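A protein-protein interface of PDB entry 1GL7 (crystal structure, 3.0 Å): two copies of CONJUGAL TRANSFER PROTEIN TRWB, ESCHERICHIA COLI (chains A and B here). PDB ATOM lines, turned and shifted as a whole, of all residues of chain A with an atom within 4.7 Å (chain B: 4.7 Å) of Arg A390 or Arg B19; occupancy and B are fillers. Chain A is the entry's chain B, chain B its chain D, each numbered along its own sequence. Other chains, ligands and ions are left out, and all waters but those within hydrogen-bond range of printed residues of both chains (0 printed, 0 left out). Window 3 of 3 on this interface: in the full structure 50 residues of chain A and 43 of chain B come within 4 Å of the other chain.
The backbone carbonyl oxygen of Arg A390 sits at hydrogen-bond distance from the guanidinium group of Arg B19.
The backbone carbonyl oxygen (O) of Val A391 sits at hydrogen-bond distance from the guanidinium group (NH2) of Arg B19, at 2.7 Å.
OE2 of Glu A396 is in salt-bridge range of NE of Arg B19, at 2.7 Å.
The backbone carbonyl oxygen of Val A392 sits at hydrogen-bond distance from the side-chain hydroxyl of Ser A357, 2.7 Å away.
The backbone carbonyl oxygen of Gly A361 sits at hydrogen-bond distance from the backbone NH of Val A391 (3.0 Å).
OE2 of Glu A362 is in salt-bridge range of NE of Arg A390.
OE2 of Glu A396 is in hydrogen-bond range of N of Met A393.
N of Leu B18 sits at hydrogen-bond distance from O of Glu B364 (2.8 Å).
The guanidinium group of Arg B19 is in salt-bridge range of the side-chain carboxylate of Glu B364, at 3.0 Å.
Among the printed residues, merely in contact across the chains: Met A393 with Arg B19 (3.3 Å), Phe A9 with Arg B19 (3.3 Å), Gly A10 with Arg B19 (3.4 Å), Gly A10 with Leu B18 (3.5 Å), Gly A11 with Arg B19 (3.5 Å), Gly A11 with Glu B364 (3.9 Å) and Val A392 with Arg B19 (3.97 Å).
Printed residues of chain B within 4 Å of Gly A10: Leu B18 (3.5 Å) and Arg B19 (3.4 Å).
Of the printed residues of chain B, Val A392 touches Arg B19 (3.97 Å).
Arg B19 touches just these residues of chain A: Phe A9, Gly A10, Gly A11, Arg A390, Val A391, Val A392, Met A393 and Glu A396.
His B363 touches none of the printed residues of chain A.
Of the printed residues of chain A, Glu B364 touches Gly A11 (3.9 Å).
The nearest printed residue of chain B that does not touch Arg A390 is Glu B364 (6.2 Å).
The nearest printed residue of chain B that does not touch Glu A396 is Gly B20 (4.4 Å).
Of the 15 printed residues of chain A, 8 touch a printed residue of chain B.
Hydrophobic or aromatic side chains of chain A within 4 Å of the printed part of chain B: Phe A9 and Met A393.
Among the printed residues, Asp or Glu carboxylates within 4 Å of a Lys or Arg side-chain nitrogen of the other chain: Glu A396 with Arg B19 (2.7 Å).
No position is printed for both chains.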
ATOM      1  N   PHE A   9     -15.338 -27.465  11.411  1.00  0.00           N
ATOM      2  CA  PHE A   9     -16.490 -27.678  10.545  1.00  0.00           C
ATOM      3  C   PHE A   9     -16.700 -26.438   9.662  1.00  0.00           C
ATOM      4  O   PHE A   9     -16.524 -25.305  10.121  1.00  0.00           O
ATOM      5  CB  PHE A   9     -17.727 -27.956  11.398  1.00  0.00           C
ATOM      6  CG  PHE A   9     -18.977 -28.170  10.603  1.00  0.00           C
ATOM      7  CD1 PHE A   9     -18.990 -29.039   9.523  1.00  0.00           C
ATOM      8  CD2 PHE A   9     -20.151 -27.515  10.945  1.00  0.00           C
ATOM      9  CE1 PHE A   9     -20.158 -29.257   8.787  1.00  0.00           C
ATOM     10  CE2 PHE A   9     -21.318 -27.723  10.219  1.00  0.00           C
ATOM     11  CZ  PHE A   9     -21.321 -28.597   9.137  1.00  0.00           C
ATOM     12  N   GLY A  10     -17.065 -26.654   8.398  1.00  0.00           N
ATOM     13  CA  GLY A  10     -17.276 -25.548   7.478  1.00  0.00           C
ATOM     14  C   GLY A  10     -18.654 -24.916   7.559  1.00  0.00           C
ATOM     15  O   GLY A  10     -18.817 -23.717   7.318  1.00  0.00           O
ATOM     16  N   GLY A  11     -19.649 -25.728   7.896  1.00  0.00           N
ATOM     17  CA  GLY A  11     -21.007 -25.235   8.002  1.00  0.00           C
ATOM     18  C   GLY A  11     -21.191 -24.386   9.239  1.00  0.00           C
ATOM     19  O   GLY A  11     -20.212 -23.938   9.841  1.00  0.00           O
ATOM     20  N   GLU A 354     -19.181 -35.449  -5.566  1.00  0.00           N
ATOM     21  CA  GLU A 354     -20.275 -35.967  -4.766  1.00  0.00           C
ATOM     22  C   GLU A 354     -19.808 -37.256  -4.074  1.00  0.00           C
ATOM     23  O   GLU A 354     -19.999 -37.423  -2.870  1.00  0.00           O
ATOM     24  CB  GLU A 354     -21.485 -36.242  -5.665  1.00  0.00           C
ATOM     25  CG  GLU A 354     -22.582 -37.083  -5.012  1.00  0.00           C
ATOM     26  CD  GLU A 354     -23.236 -36.413  -3.829  1.00  0.00           C
ATOM     27  OE1 GLU A 354     -24.016 -37.096  -3.132  1.00  0.00           O
ATOM     28  OE2 GLU A 354     -22.975 -35.213  -3.603  1.00  0.00           O
ATOM     29  N   SER A 357     -17.529 -36.344  -1.306  1.00  0.00           N
ATOM     30  CA  SER A 357     -18.302 -35.668  -0.270  1.00  0.00           C
ATOM     31  C   SER A 357     -19.024 -36.697   0.589  1.00  0.00           C
ATOM     32  O   SER A 357     -19.073 -36.590   1.819  1.00  0.00           O
ATOM     33  CB  SER A 357     -19.332 -34.723  -0.909  1.00  0.00           C
ATOM     34  OG  SER A 357     -20.254 -34.190   0.041  1.00  0.00           O
ATOM     35  N   LEU A 358     -19.572 -37.700  -0.081  1.00  0.00           N
ATOM     36  CA  LEU A 358     -20.321 -38.750   0.573  1.00  0.00           C
ATOM     37  C   LEU A 358     -19.394 -39.762   1.251  1.00  0.00           C
ATOM     38  O   LEU A 358     -19.726 -40.316   2.294  1.00  0.00           O
ATOM     39  CB  LEU A 358     -21.214 -39.419  -0.465  1.00  0.00           C
ATOM     40  CG  LEU A 358     -22.404 -40.247   0.007  1.00  0.00           C
ATOM     41  CD1 LEU A 358     -23.232 -40.697  -1.196  1.00  0.00           C
ATOM     42  CD2 LEU A 358     -21.891 -41.442   0.778  1.00  0.00           C
ATOM     43  N   GLY A 361     -18.616 -38.568   4.439  1.00  0.00           N
ATOM     44  CA  GLY A 361     -19.692 -38.764   5.392  1.00  0.00           C
ATOM     45  C   GLY A 361     -20.498 -37.580   5.884  1.00  0.00           C
ATOM     46  O   GLY A 361     -20.133 -36.411   5.663  1.00  0.00           O
ATOM     47  N   GLU A 362     -21.616 -37.908   6.543  1.00  0.00           N
ATOM     48  CA  GLU A 362     -22.538 -36.936   7.136  1.00  0.00           C
ATOM     49  C   GLU A 362     -22.421 -37.034   8.659  1.00  0.00           C
ATOM     50  O   GLU A 362     -21.771 -37.932   9.197  1.00  0.00           O
ATOM     51  CB  GLU A 362     -24.007 -37.238   6.770  1.00  0.00           C
ATOM     52  CG  GLU A 362     -24.424 -37.096   5.300  1.00  0.00           C
ATOM     53  CD  GLU A 362     -25.954 -37.127   5.129  1.00  0.00           C
ATOM     54  OE1 GLU A 362     -26.609 -37.888   5.877  1.00  0.00           O
ATOM     55  OE2 GLU A 362     -26.499 -36.405   4.254  1.00  0.00           O
ATOM     56  N   GLU A 389     -26.280 -33.692   7.933  1.00  0.00           N
ATOM     57  CA  GLU A 389     -25.628 -33.049   6.804  1.00  0.00           C
ATOM     58  C   GLU A 389     -24.217 -33.499   6.472  1.00  0.00           C
ATOM     59  O   GLU A 389     -23.528 -34.084   7.299  1.00  0.00           O
ATOM     60  CB  GLU A 389     -25.619 -31.557   7.038  1.00  0.00           C
ATOM     61  CG  GLU A 389     -25.390 -31.211   8.470  1.00  0.00           C
ATOM     62  CD  GLU A 389     -25.385 -29.728   8.685  1.00  0.00           C
ATOM     63  OE1 GLU A 389     -26.272 -29.042   8.132  1.00  0.00           O
ATOM     64  OE2 GLU A 389     -24.498 -29.238   9.408  1.00  0.00           O
ATOM     65  N   ARG A 390     -23.786 -33.209   5.251  1.00  0.00           N
ATOM     66  CA  ARG A 390     -22.450 -33.582   4.828  1.00  0.00           C
ATOM     67  C   ARG A 390     -21.463 -32.765   5.616  1.00  0.00           C
ATOM     68  O   ARG A 390     -21.628 -31.544   5.761  1.00  0.00           O
ATOM     69  CB  ARG A 390     -22.225 -33.288   3.346  1.00  0.00           C
ATOM     70  CG  ARG A 390     -23.099 -34.070   2.388  1.00  0.00           C
ATOM     71  CD  ARG A 390     -22.960 -35.556   2.580  1.00  0.00           C
ATOM     72  NE  ARG A 390     -23.833 -36.288   1.670  1.00  0.00           N
ATOM     73  CZ  ARG A 390     -23.609 -36.408   0.368  1.00  0.00           C
ATOM     74  NH1 ARG A 390     -22.537 -35.846  -0.171  1.00  0.00           N
ATOM     75  NH2 ARG A 390     -24.445 -37.095  -0.395  1.00  0.00           N
ATOM     76  N   VAL A 391     -20.446 -33.451   6.133  1.00  0.00           N
ATOM     77  CA  VAL A 391     -19.379 -32.805   6.885  1.00  0.00           C
ATOM     78  C   VAL A 391     -18.633 -31.910   5.896  1.00  0.00           C
ATOM     79  O   VAL A 391     -18.297 -30.760   6.198  1.00  0.00           O
ATOM     80  CB  VAL A 391     -18.422 -33.857   7.498  1.00  0.00           C
ATOM     81  CG1 VAL A 391     -17.211 -33.161   8.115  1.00  0.00           C
ATOM     82  CG2 VAL A 391     -19.167 -34.688   8.556  1.00  0.00           C
ATOM     83  N   VAL A 392     -18.385 -32.446   4.701  1.00  0.00           N
ATOM     84  CA  VAL A 392     -17.731 -31.666   3.659  1.00  0.00           C
ATOM     85  C   VAL A 392     -18.620 -31.711   2.433  1.00  0.00           C
ATOM     86  O   VAL A 392     -18.965 -32.792   1.955  1.00  0.00           O
ATOM     87  CB  VAL A 392     -16.348 -32.213   3.270  1.00  0.00           C
ATOM     88  CG1 VAL A 392     -15.674 -31.228   2.301  1.00  0.00           C
ATOM     89  CG2 VAL A 392     -15.485 -32.415   4.521  1.00  0.00           C
ATOM     90  N   MET A 393     -19.000 -30.529   1.953  1.00  0.00           N
ATOM     91  CA  MET A 393     -19.848 -30.398   0.784  1.00  0.00           C
ATOM     92  C   MET A 393     -19.050 -30.707  -0.457  1.00  0.00           C
ATOM     93  O   MET A 393     -17.828 -30.599  -0.456  1.00  0.00           O
ATOM     94  CB  MET A 393     -20.379 -28.978   0.686  1.00  0.00           C
ATOM     95  CG  MET A 393     -21.613 -28.737   1.514  1.00  0.00           C
ATOM     96  SD  MET A 393     -22.244 -27.065   1.287  1.00  0.00           S
ATOM     97  CE  MET A 393     -22.537 -27.067  -0.548  1.00  0.00           C
ATOM     98  N   PRO A 394     -19.725 -31.107  -1.541  1.00  0.00           N
ATOM     99  CA  PRO A 394     -18.971 -31.403  -2.756  1.00  0.00           C
ATOM    100  C   PRO A 394     -18.305 -30.100  -3.187  1.00  0.00           C
ATOM    101  O   PRO A 394     -17.163 -30.086  -3.662  1.00  0.00           O
ATOM    102  CB  PRO A 394     -20.056 -31.850  -3.725  1.00  0.00           C
ATOM    103  CG  PRO A 394     -21.089 -32.438  -2.829  1.00  0.00           C
ATOM    104  CD  PRO A 394     -21.144 -31.444  -1.714  1.00  0.00           C
ATOM    105  N   GLU A 396     -17.123 -27.667  -1.391  1.00  0.00           N
ATOM    106  CA  GLU A 396     -15.894 -27.430  -0.641  1.00  0.00           C
ATOM    107  C   GLU A 396     -14.709 -28.139  -1.295  1.00  0.00           C
ATOM    108  O   GLU A 396     -13.616 -27.576  -1.414  1.00  0.00           O
ATOM    109  CB  GLU A 396     -16.074 -27.903   0.809  1.00  0.00           C
ATOM    110  CG  GLU A 396     -17.332 -27.343   1.467  1.00  0.00           C
ATOM    111  CD  GLU A 396     -17.329 -27.491   2.970  1.00  0.00           C
ATOM    112  OE1 GLU A 396     -16.409 -26.957   3.620  1.00  0.00           O
ATOM    113  OE2 GLU A 396     -18.250 -28.133   3.508  1.00  0.00           O
ATOM    114  N   PHE B  17     -22.503 -15.928   4.653  1.00  0.00           N
ATOM    115  CA  PHE B  17     -22.066 -17.073   3.862  1.00  0.00           C
ATOM    116  C   PHE B  17     -21.317 -18.059   4.734  1.00  0.00           C
ATOM    117  O   PHE B  17     -20.366 -17.696   5.438  1.00  0.00           O
ATOM    118  CB  PHE B  17     -21.163 -16.620   2.717  1.00  0.00           C
ATOM    119  CG  PHE B  17     -20.509 -17.752   1.957  1.00  0.00           C
ATOM    120  CD1 PHE B  17     -19.378 -18.394   2.461  1.00  0.00           C
ATOM    121  CD2 PHE B  17     -21.023 -18.169   0.729  1.00  0.00           C
ATOM    122  CE1 PHE B  17     -18.763 -19.420   1.753  1.00  0.00           C
ATOM    123  CE2 PHE B  17     -20.413 -19.197   0.014  1.00  0.00           C
ATOM    124  CZ  PHE B  17     -19.280 -19.826   0.531  1.00  0.00           C
ATOM    125  N   LEU B  18     -21.735 -19.317   4.664  1.00  0.00           N
ATOM    126  CA  LEU B  18     -21.110 -20.362   5.452  1.00  0.00           C
ATOM    127  C   LEU B  18     -20.032 -21.110   4.696  1.00  0.00           C
ATOM    128  O   LEU B  18     -18.859 -21.025   5.050  1.00  0.00           O
ATOM    129  CB  LEU B  18     -22.165 -21.350   5.940  1.00  0.00           C
ATOM    130  CG  LEU B  18     -23.304 -20.679   6.702  1.00  0.00           C
ATOM    131  CD1 LEU B  18     -24.252 -21.712   7.274  1.00  0.00           C
ATOM    132  CD2 LEU B  18     -22.710 -19.832   7.816  1.00  0.00           C
ATOM    133  N   ARG B  19     -20.443 -21.834   3.657  1.00  0.00           N
ATOM    134  CA  ARG B  19     -19.520 -22.644   2.873  1.00  0.00           C
ATOM    135  C   ARG B  19     -20.030 -22.897   1.477  1.00  0.00           C
ATOM    136  O   ARG B  19     -21.182 -22.608   1.164  1.00  0.00           O
ATOM    137  CB  ARG B  19     -19.304 -23.991   3.568  1.00  0.00           C
ATOM    138  CG  ARG B  19     -20.491 -24.367   4.434  1.00  0.00           C
ATOM    139  CD  ARG B  19     -21.107 -25.701   4.098  1.00  0.00           C
ATOM    140  NE  ARG B  19     -20.333 -26.823   4.608  1.00  0.00           N
ATOM    141  CZ  ARG B  19     -20.876 -27.955   5.051  1.00  0.00           C
ATOM    142  NH1 ARG B  19     -22.196 -28.110   5.055  1.00  0.00           N
ATOM    143  NH2 ARG B  19     -20.097 -28.947   5.475  1.00  0.00           N
ATOM    144  N   GLY B  20     -19.151 -23.452   0.642  1.00  0.00           N
ATOM    145  CA  GLY B  20     -19.502 -23.764  -0.733  1.00  0.00           C
ATOM    146  C   GLY B  20     -18.945 -22.818  -1.787  1.00  0.00           C
ATOM    147  O   GLY B  20     -17.943 -22.123  -1.573  1.00  0.00           O
ATOM    148  N   THR B  21     -19.597 -22.805  -2.948  1.00  0.00           N
ATOM    149  CA  THR B  21     -19.181 -21.941  -4.044  1.00  0.00           C
ATOM    150  C   THR B  21     -19.602 -20.501  -3.754  1.00  0.00           C
ATOM    151  O   THR B  21     -20.687 -20.244  -3.234  1.00  0.00           O
ATOM    152  CB  THR B  21     -19.793 -22.417  -5.392  1.00  0.00           C
ATOM    153  OG1 THR B  21     -19.195 -23.659  -5.778  1.00  0.00           O
ATOM    154  CG2 THR B  21     -19.554 -21.388  -6.492  1.00  0.00           C
ATOM    155  N   HIS B 363     -24.022 -23.519  -2.345  1.00  0.00           N
ATOM    156  CA  HIS B 363     -23.408 -22.777  -1.253  1.00  0.00           C
ATOM    157  C   HIS B 363     -24.315 -22.938  -0.043  1.00  0.00           C
ATOM    158  O   HIS B 363     -25.490 -23.273  -0.186  1.00  0.00           O
ATOM    159  CB  HIS B 363     -23.276 -21.288  -1.616  1.00  0.00           C
ATOM    160  CG  HIS B 363     -24.584 -20.548  -1.706  1.00  0.00           C
ATOM    161  ND1 HIS B 363     -24.662 -19.230  -2.089  1.00  0.00           N
ATOM    162  CD2 HIS B 363     -25.856 -20.937  -1.428  1.00  0.00           C
ATOM    163  CE1 HIS B 363     -25.926 -18.831  -2.041  1.00  0.00           C
ATOM    164  NE2 HIS B 363     -26.666 -19.848  -1.643  1.00  0.00           N
ATOM    165  N   GLU B 364     -23.782 -22.745   1.152  1.00  0.00           N
ATOM    166  CA  GLU B 364     -24.642 -22.827   2.308  1.00  0.00           C
ATOM    167  C   GLU B 364     -24.616 -21.430   2.882  1.00  0.00           C
ATOM    168  O   GLU B 364     -23.551 -20.848   3.130  1.00  0.00           O
ATOM    169  CB  GLU B 364     -24.149 -23.857   3.298  1.00  0.00           C
ATOM    170  CG  GLU B 364     -25.266 -24.354   4.170  1.00  0.00           C
ATOM    171  CD  GLU B 364     -24.942 -25.677   4.794  1.00  0.00           C
ATOM    172  OE1 GLU B 364     -23.915 -25.744   5.502  1.00  0.00           O
ATOM    173  OE2 GLU B 364     -25.708 -26.647   4.572  1.00  0.00           O
